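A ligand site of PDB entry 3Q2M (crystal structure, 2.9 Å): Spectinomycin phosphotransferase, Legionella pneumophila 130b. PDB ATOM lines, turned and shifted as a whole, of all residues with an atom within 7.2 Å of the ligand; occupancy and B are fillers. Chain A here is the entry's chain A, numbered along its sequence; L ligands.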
ATOM      1  N   ILE A  29     -32.743  -5.239  16.790  1.00  0.00           N
ATOM      2  CA  ILE A  29     -32.904  -5.620  15.387  1.00  0.00           C
ATOM      3  C   ILE A  29     -32.083  -6.862  15.079  1.00  0.00           C
ATOM      4  O   ILE A  29     -30.906  -6.957  15.461  1.00  0.00           O
ATOM      5  CB  ILE A  29     -32.461  -4.481  14.453  1.00  0.00           C
ATOM      6  CG1 ILE A  29     -33.305  -3.239  14.726  1.00  0.00           C
ATOM      7  CG2 ILE A  29     -32.596  -4.912  13.008  1.00  0.00           C
ATOM      8  CD1 ILE A  29     -32.684  -1.959  14.223  1.00  0.00           C
ATOM      9  N   GLY A  31     -29.794  -8.344  13.354  1.00  0.00           N
ATOM     10  CA  GLY A  31     -28.661  -8.234  12.431  1.00  0.00           C
ATOM     11  C   GLY A  31     -28.262  -6.862  11.905  1.00  0.00           C
ATOM     12  O   GLY A  31     -27.934  -5.954  12.674  1.00  0.00           O
ATOM     13  N   GLY A  32     -28.264  -6.736  10.581  1.00  0.00           N
ATOM     14  CA  GLY A  32     -27.865  -5.502   9.920  1.00  0.00           C
ATOM     15  C   GLY A  32     -26.563  -5.758   9.176  1.00  0.00           C
ATOM     16  O   GLY A  32     -26.576  -6.223   8.031  1.00  0.00           O
ATOM     17  N   ALA A  33     -25.452  -5.470   9.853  1.00  0.00           N
ATOM     18  CA  ALA A  33     -24.103  -5.671   9.306  1.00  0.00           C
ATOM     19  C   ALA A  33     -23.265  -6.319  10.418  1.00  0.00           C
ATOM     20  O   ALA A  33     -22.606  -5.623  11.200  1.00  0.00           O
ATOM     21  CB  ALA A  33     -23.485  -4.341   8.881  1.00  0.00           C
ATOM     22  N   ALA A  39     -27.568  -4.421  16.687  1.00  0.00           N
ATOM     23  CA  ALA A  39     -28.168  -3.116  16.540  1.00  0.00           C
ATOM     24  C   ALA A  39     -29.488  -2.997  17.245  1.00  0.00           C
ATOM     25  O   ALA A  39     -30.238  -3.954  17.332  1.00  0.00           O
ATOM     26  CB  ALA A  39     -28.344  -2.796  15.068  1.00  0.00           C
ATOM     27  N   GLN A  41     -32.857   0.017  17.995  1.00  0.00           N
ATOM     28  CA  GLN A  41     -33.506   1.257  17.618  1.00  0.00           C
ATOM     29  C   GLN A  41     -34.088   1.872  18.879  1.00  0.00           C
ATOM     30  O   GLN A  41     -35.202   1.537  19.284  1.00  0.00           O
ATOM     31  CB  GLN A  41     -34.635   1.031  16.624  1.00  0.00           C
ATOM     32  CG  GLN A  41     -35.205   2.356  16.120  1.00  0.00           C
ATOM     33  CD  GLN A  41     -36.512   2.203  15.376  1.00  0.00           C
ATOM     34  OE1 GLN A  41     -36.671   1.282  14.573  1.00  0.00           O
ATOM     35  NE2 GLN A  41     -37.447   3.111  15.633  1.00  0.00           N
ATOM     36  N   TYR A  49     -32.810   6.819  17.326  1.00  0.00           N
ATOM     37  CA  TYR A  49     -31.372   6.664  17.176  1.00  0.00           C
ATOM     38  C   TYR A  49     -31.072   5.244  16.786  1.00  0.00           C
ATOM     39  O   TYR A  49     -31.841   4.336  17.087  1.00  0.00           O
ATOM     40  CB  TYR A  49     -30.669   6.964  18.480  1.00  0.00           C
ATOM     41  CG  TYR A  49     -30.799   8.394  18.937  1.00  0.00           C
ATOM     42  CD1 TYR A  49     -29.859   9.350  18.576  1.00  0.00           C
ATOM     43  CD2 TYR A  49     -31.866   8.791  19.756  1.00  0.00           C
ATOM     44  CE1 TYR A  49     -29.953  10.660  19.010  1.00  0.00           C
ATOM     45  CE2 TYR A  49     -31.973  10.103  20.190  1.00  0.00           C
ATOM     46  CZ  TYR A  49     -31.010  11.031  19.822  1.00  0.00           C
ATOM     47  OH  TYR A  49     -31.113  12.330  20.253  1.00  0.00           O
ATOM     48  N   PHE A  50     -29.943   5.057  16.095  1.00  0.00           N
ATOM     49  CA  PHE A  50     -29.514   3.726  15.696  1.00  0.00           C
ATOM     50  C   PHE A  50     -28.333   3.433  16.583  1.00  0.00           C
ATOM     51  O   PHE A  50     -27.295   4.086  16.504  1.00  0.00           O
ATOM     52  CB  PHE A  50     -29.101   3.710  14.230  1.00  0.00           C
ATOM     53  CG  PHE A  50     -28.628   2.363  13.744  1.00  0.00           C
ATOM     54  CD1 PHE A  50     -27.258   2.081  13.664  1.00  0.00           C
ATOM     55  CD2 PHE A  50     -29.532   1.407  13.298  1.00  0.00           C
ATOM     56  CE1 PHE A  50     -26.809   0.868  13.134  1.00  0.00           C
ATOM     57  CE2 PHE A  50     -29.090   0.190  12.772  1.00  0.00           C
ATOM     58  CZ  PHE A  50     -27.717  -0.076  12.691  1.00  0.00           C
ATOM     59  N   ILE A  51     -28.515   2.453  17.464  1.00  0.00           N
ATOM     60  CA  ILE A  51     -27.473   2.087  18.399  1.00  0.00           C
ATOM     61  C   ILE A  51     -26.766   0.842  17.955  1.00  0.00           C
ATOM     62  O   ILE A  51     -27.389  -0.111  17.520  1.00  0.00           O
ATOM     63  CB  ILE A  51     -28.032   1.851  19.776  1.00  0.00           C
ATOM     64  CG1 ILE A  51     -29.090   2.920  20.079  1.00  0.00           C
ATOM     65  CG2 ILE A  51     -26.895   1.867  20.791  1.00  0.00           C
ATOM     66  CD1 ILE A  51     -28.609   4.322  19.844  1.00  0.00           C
ATOM     67  N   LYS A  52     -25.467   0.849  18.106  1.00  0.00           N
ATOM     68  CA  LYS A  52     -24.678  -0.295  17.691  1.00  0.00           C
ATOM     69  C   LYS A  52     -23.742  -0.704  18.830  1.00  0.00           C
ATOM     70  O   LYS A  52     -23.105   0.156  19.450  1.00  0.00           O
ATOM     71  CB  LYS A  52     -23.893   0.099  16.429  1.00  0.00           C
ATOM     72  CG  LYS A  52     -23.117  -1.007  15.744  1.00  0.00           C
ATOM     73  CD  LYS A  52     -22.230  -0.425  14.633  1.00  0.00           C
ATOM     74  CE  LYS A  52     -23.047   0.333  13.584  1.00  0.00           C
ATOM     75  NZ  LYS A  52     -22.202   0.837  12.443  1.00  0.00           N
ATOM     76  N   ILE A  78     -23.341   9.061   7.495  1.00  0.00           N
ATOM     77  CA  ILE A  78     -24.014   9.122   8.783  1.00  0.00           C
ATOM     78  C   ILE A  78     -23.009   9.384   9.917  1.00  0.00           C
ATOM     79  O   ILE A  78     -22.258   8.492  10.293  1.00  0.00           O
ATOM     80  CB  ILE A  78     -24.737   7.804   9.057  1.00  0.00           C
ATOM     81  CG1 ILE A  78     -25.673   7.492   7.887  1.00  0.00           C
ATOM     82  CG2 ILE A  78     -25.487   7.905  10.379  1.00  0.00           C
ATOM     83  CD1 ILE A  78     -26.395   6.180   8.008  1.00  0.00           C
ATOM     84  N   TYR A 100     -26.055   6.401  16.379  1.00  0.00           N
ATOM     85  CA  TYR A 100     -26.190   7.166  15.156  1.00  0.00           C
ATOM     86  C   TYR A 100     -27.612   7.652  15.082  1.00  0.00           C
ATOM     87  O   TYR A 100     -28.512   7.044  15.670  1.00  0.00           O
ATOM     88  CB  TYR A 100     -25.964   6.300  13.926  1.00  0.00           C
ATOM     89  CG  TYR A 100     -24.569   5.770  13.721  1.00  0.00           C
ATOM     90  CD1 TYR A 100     -24.078   4.723  14.495  1.00  0.00           C
ATOM     91  CD2 TYR A 100     -23.742   6.299  12.735  1.00  0.00           C
ATOM     92  CE1 TYR A 100     -22.788   4.209  14.283  1.00  0.00           C
ATOM     93  CE2 TYR A 100     -22.457   5.803  12.509  1.00  0.00           C
ATOM     94  CZ  TYR A 100     -21.994   4.760  13.284  1.00  0.00           C
ATOM     95  OH  TYR A 100     -20.728   4.278  13.062  1.00  0.00           O
ATOM     96  N   PRO A 101     -27.837   8.765  14.389  1.00  0.00           N
ATOM     97  CA  PRO A 101     -29.231   9.210  14.306  1.00  0.00           C
ATOM     98  C   PRO A 101     -29.887   8.185  13.379  1.00  0.00           C
ATOM     99  O   PRO A 101     -29.342   7.858  12.318  1.00  0.00           O
ATOM    100  CB  PRO A 101     -29.118  10.608  13.703  1.00  0.00           C
ATOM    101  CG  PRO A 101     -27.857  10.548  12.918  1.00  0.00           C
ATOM    102  CD  PRO A 101     -26.930   9.765  13.795  1.00  0.00           C
ATOM    103  N   PHE A 102     -31.026   7.651  13.801  1.00  0.00           N
ATOM    104  CA  PHE A 102     -31.730   6.643  13.016  1.00  0.00           C
ATOM    105  C   PHE A 102     -32.206   7.122  11.636  1.00  0.00           C
ATOM    106  O   PHE A 102     -32.716   8.235  11.490  1.00  0.00           O
ATOM    107  CB  PHE A 102     -32.937   6.129  13.793  1.00  0.00           C
ATOM    108  CG  PHE A 102     -33.508   4.867  13.243  1.00  0.00           C
ATOM    109  CD1 PHE A 102     -33.056   3.630  13.680  1.00  0.00           C
ATOM    110  CD2 PHE A 102     -34.463   4.915  12.219  1.00  0.00           C
ATOM    111  CE1 PHE A 102     -33.541   2.458  13.115  1.00  0.00           C
ATOM    112  CE2 PHE A 102     -34.948   3.747  11.637  1.00  0.00           C
ATOM    113  CZ  PHE A 102     -34.487   2.516  12.094  1.00  0.00           C
ATOM    114  N   ILE A 103     -32.041   6.262  10.639  1.00  0.00           N
ATOM    115  CA  ILE A 103     -32.452   6.568   9.277  1.00  0.00           C
ATOM    116  C   ILE A 103     -33.342   5.471   8.696  1.00  0.00           C
ATOM    117  O   ILE A 103     -32.906   4.327   8.562  1.00  0.00           O
ATOM    118  CB  ILE A 103     -31.230   6.702   8.331  1.00  0.00           C
ATOM    119  CG1 ILE A 103     -30.257   7.761   8.849  1.00  0.00           C
ATOM    120  CG2 ILE A 103     -31.710   6.995   6.913  1.00  0.00           C
ATOM    121  CD1 ILE A 103     -30.857   9.108   9.038  1.00  0.00           C
ATOM    122  N   HIS A 104     -34.591   5.813   8.368  1.00  0.00           N
ATOM    123  CA  HIS A 104     -35.489   4.849   7.742  1.00  0.00           C
ATOM    124  C   HIS A 104     -35.207   5.114   6.284  1.00  0.00           C
ATOM    125  O   HIS A 104     -35.386   6.238   5.813  1.00  0.00           O
ATOM    126  CB  HIS A 104     -36.956   5.198   7.968  1.00  0.00           C
ATOM    127  CG  HIS A 104     -37.320   5.349   9.402  1.00  0.00           C
ATOM    128  ND1 HIS A 104     -37.978   4.356  10.104  1.00  0.00           N
ATOM    129  CD2 HIS A 104     -37.127   6.367  10.275  1.00  0.00           C
ATOM    130  CE1 HIS A 104     -38.171   4.765  11.349  1.00  0.00           C
ATOM    131  NE2 HIS A 104     -37.670   5.980  11.472  1.00  0.00           N
ATOM    132  N   ALA A 105     -34.740   4.101   5.564  1.00  0.00           N
ATOM    133  CA  ALA A 105     -34.440   4.292   4.154  1.00  0.00           C
ATOM    134  C   ALA A 105     -34.032   2.975   3.574  1.00  0.00           C
ATOM    135  O   ALA A 105     -32.971   2.456   3.891  1.00  0.00           O
ATOM    136  CB  ALA A 105     -33.303   5.308   3.984  1.00  0.00           C
ATOM    137  N   PRO A 106     -34.880   2.418   2.719  1.00  0.00           N
ATOM    138  CA  PRO A 106     -34.538   1.137   2.107  1.00  0.00           C
ATOM    139  C   PRO A 106     -33.127   1.225   1.553  1.00  0.00           C
ATOM    140  O   PRO A 106     -32.721   2.288   1.064  1.00  0.00           O
ATOM    141  CB  PRO A 106     -35.563   1.010   0.994  1.00  0.00           C
ATOM    142  CG  PRO A 106     -35.735   2.456   0.576  1.00  0.00           C
ATOM    143  CD  PRO A 106     -35.890   3.111   1.922  1.00  0.00           C
ATOM    144  N   ASN A 107     -32.363   0.142   1.651  1.00  0.00           N
ATOM    145  CA  ASN A 107     -31.025   0.181   1.086  1.00  0.00           C
ATOM    146  C   ASN A 107     -31.163   0.014  -0.427  1.00  0.00           C
ATOM    147  O   ASN A 107     -32.272   0.004  -0.971  1.00  0.00           O
ATOM    148  CB  ASN A 107     -30.140  -0.903   1.670  1.00  0.00           C
ATOM    149  CG  ASN A 107     -30.692  -2.276   1.479  1.00  0.00           C
ATOM    150  OD1 ASN A 107     -31.036  -2.672   0.364  1.00  0.00           O
ATOM    151  ND2 ASN A 107     -30.790  -3.025   2.558  1.00  0.00           N
ATOM    152  N   GLY A 216     -25.993  -2.644  -1.395  1.00  0.00           N
ATOM    153  CA  GLY A 216     -26.329  -2.956  -0.020  1.00  0.00           C
ATOM    154  C   GLY A 216     -25.905  -1.870   0.964  1.00  0.00           C
ATOM    155  O   GLY A 216     -26.465  -1.772   2.053  1.00  0.00           O
ATOM    156  N   LEU A 219     -27.946   3.894   1.277  1.00  0.00           N
ATOM    157  CA  LEU A 219     -29.294   4.022   1.806  1.00  0.00           C
ATOM    158  C   LEU A 219     -29.918   5.078   0.916  1.00  0.00           C
ATOM    159  O   LEU A 219     -29.458   6.217   0.874  1.00  0.00           O
ATOM    160  CB  LEU A 219     -29.269   4.478   3.263  1.00  0.00           C
ATOM    161  CG  LEU A 219     -28.684   3.461   4.246  1.00  0.00           C
ATOM    162  CD1 LEU A 219     -29.123   3.812   5.668  1.00  0.00           C
ATOM    163  CD2 LEU A 219     -29.154   2.068   3.883  1.00  0.00           C
ATOM    164  N   ILE A 229     -23.141   3.957   3.939  1.00  0.00           N
ATOM    165  CA  ILE A 229     -22.830   3.366   5.233  1.00  0.00           C
ATOM    166  C   ILE A 229     -21.744   2.279   5.181  1.00  0.00           C
ATOM    167  O   ILE A 229     -21.220   1.913   4.117  1.00  0.00           O
ATOM    168  CB  ILE A 229     -24.083   2.752   5.838  1.00  0.00           C
ATOM    169  CG1 ILE A 229     -24.501   1.521   5.045  1.00  0.00           C
ATOM    170  CG2 ILE A 229     -25.214   3.766   5.802  1.00  0.00           C
ATOM    171  CD1 ILE A 229     -25.731   0.848   5.577  1.00  0.00           C
ATOM    172  N   ASP A 230     -21.434   1.753   6.366  1.00  0.00           N
ATOM    173  CA  ASP A 230     -20.446   0.702   6.554  1.00  0.00           C
ATOM    174  C   ASP A 230     -19.045   1.113   6.190  1.00  0.00           C
ATOM    175  O   ASP A 230     -18.593   0.888   5.071  1.00  0.00           O
ATOM    176  CB  ASP A 230     -20.791  -0.572   5.798  1.00  0.00           C
ATOM    177  CG  ASP A 230     -19.965  -1.766   6.262  1.00  0.00           C
ATOM    178  OD1 ASP A 230     -18.718  -1.733   6.093  1.00  0.00           O
ATOM    179  OD2 ASP A 230     -20.559  -2.726   6.829  1.00  0.00           O
HETATM  180  C1  LIG L   1     -30.302   3.134  10.308  1.00  0.00           C
HETATM  181  N1  LIG L   1     -29.983   4.388  10.845  1.00  0.00           N
HETATM  182  C2  LIG L   1     -28.627   4.713  10.924  1.00  0.00           C
HETATM  183  C3  LIG L   1     -27.572   3.837  10.495  1.00  0.00           C
HETATM  184  C4  LIG L   1     -26.892   1.630   9.499  1.00  0.00           C
HETATM  185 CL1  LIG L   1     -25.213   1.998   9.587  1.00  0.00          CL
HETATM  186  C5  LIG L   1     -27.264   0.355   8.962  1.00  0.00           C
HETATM  187  C6  LIG L   1     -28.644  -0.021   8.866  1.00  0.00           C
HETATM  188  C7  LIG L   1     -29.681   0.876   9.299  1.00  0.00           C
HETATM  189  C8  LIG L   1     -29.317   2.183   9.850  1.00  0.00           C
HETATM  190  C9  LIG L   1     -27.917   2.551   9.950  1.00  0.00           C
HETATM  191  S1  LIG L   1     -31.379   0.289   9.123  1.00  0.00           S
HETATM  192  O1  LIG L   1     -31.711  -0.356  10.371  1.00  0.00           O
HETATM  193  O2  LIG L   1     -31.359  -0.644   8.044  1.00  0.00           O
HETATM  194  N2  LIG L   1     -32.506   1.561   8.863  1.00  0.00           N
HETATM  195  C10 LIG L   1     -33.394   1.639   7.627  1.00  0.00           C
HETATM  196  C11 LIG L   1     -33.342   0.625   6.451  1.00  0.00           C
HETATM  197  N3  LIG L   1     -32.014   0.093   6.181  1.00  0.00           N
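The backbone NH (N) of Ile 103 is in hydrogen-bond range of a nitrogen (N1) of the ligand, 2.8 Å away. O of Ala 105 sits close to N3 of the ligand (3.4 Å). O of Ile 103 lies within hydrogen-bond range of N2 of the ligand (2.8 Å).
The backbone NH (N) of Phe 50 lies within hydrogen-bond range of the backbone carbonyl oxygen (O) of Tyr 100, at 2.5 Å.
Phe 50 touches the ligand. Ile 78 touches the ligand. Pro 101 touches the ligand (O to C2, 3.5 Å). CA of Phe 102 touches N1 of the ligand, 3.6 Å away. His 104 touches the ligand (CA to C10, 3.8 Å). Ile 229 touches the ligand (CD1 to C5, 3.7 Å). Hydrophobic or aromatic side chains within 4 Å of the ligand: Phe 50, Ile 78, Phe 102, Ile 103 and Ile 229. Of the 23 residues printed, 8 come within 4 Å of the ligand.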
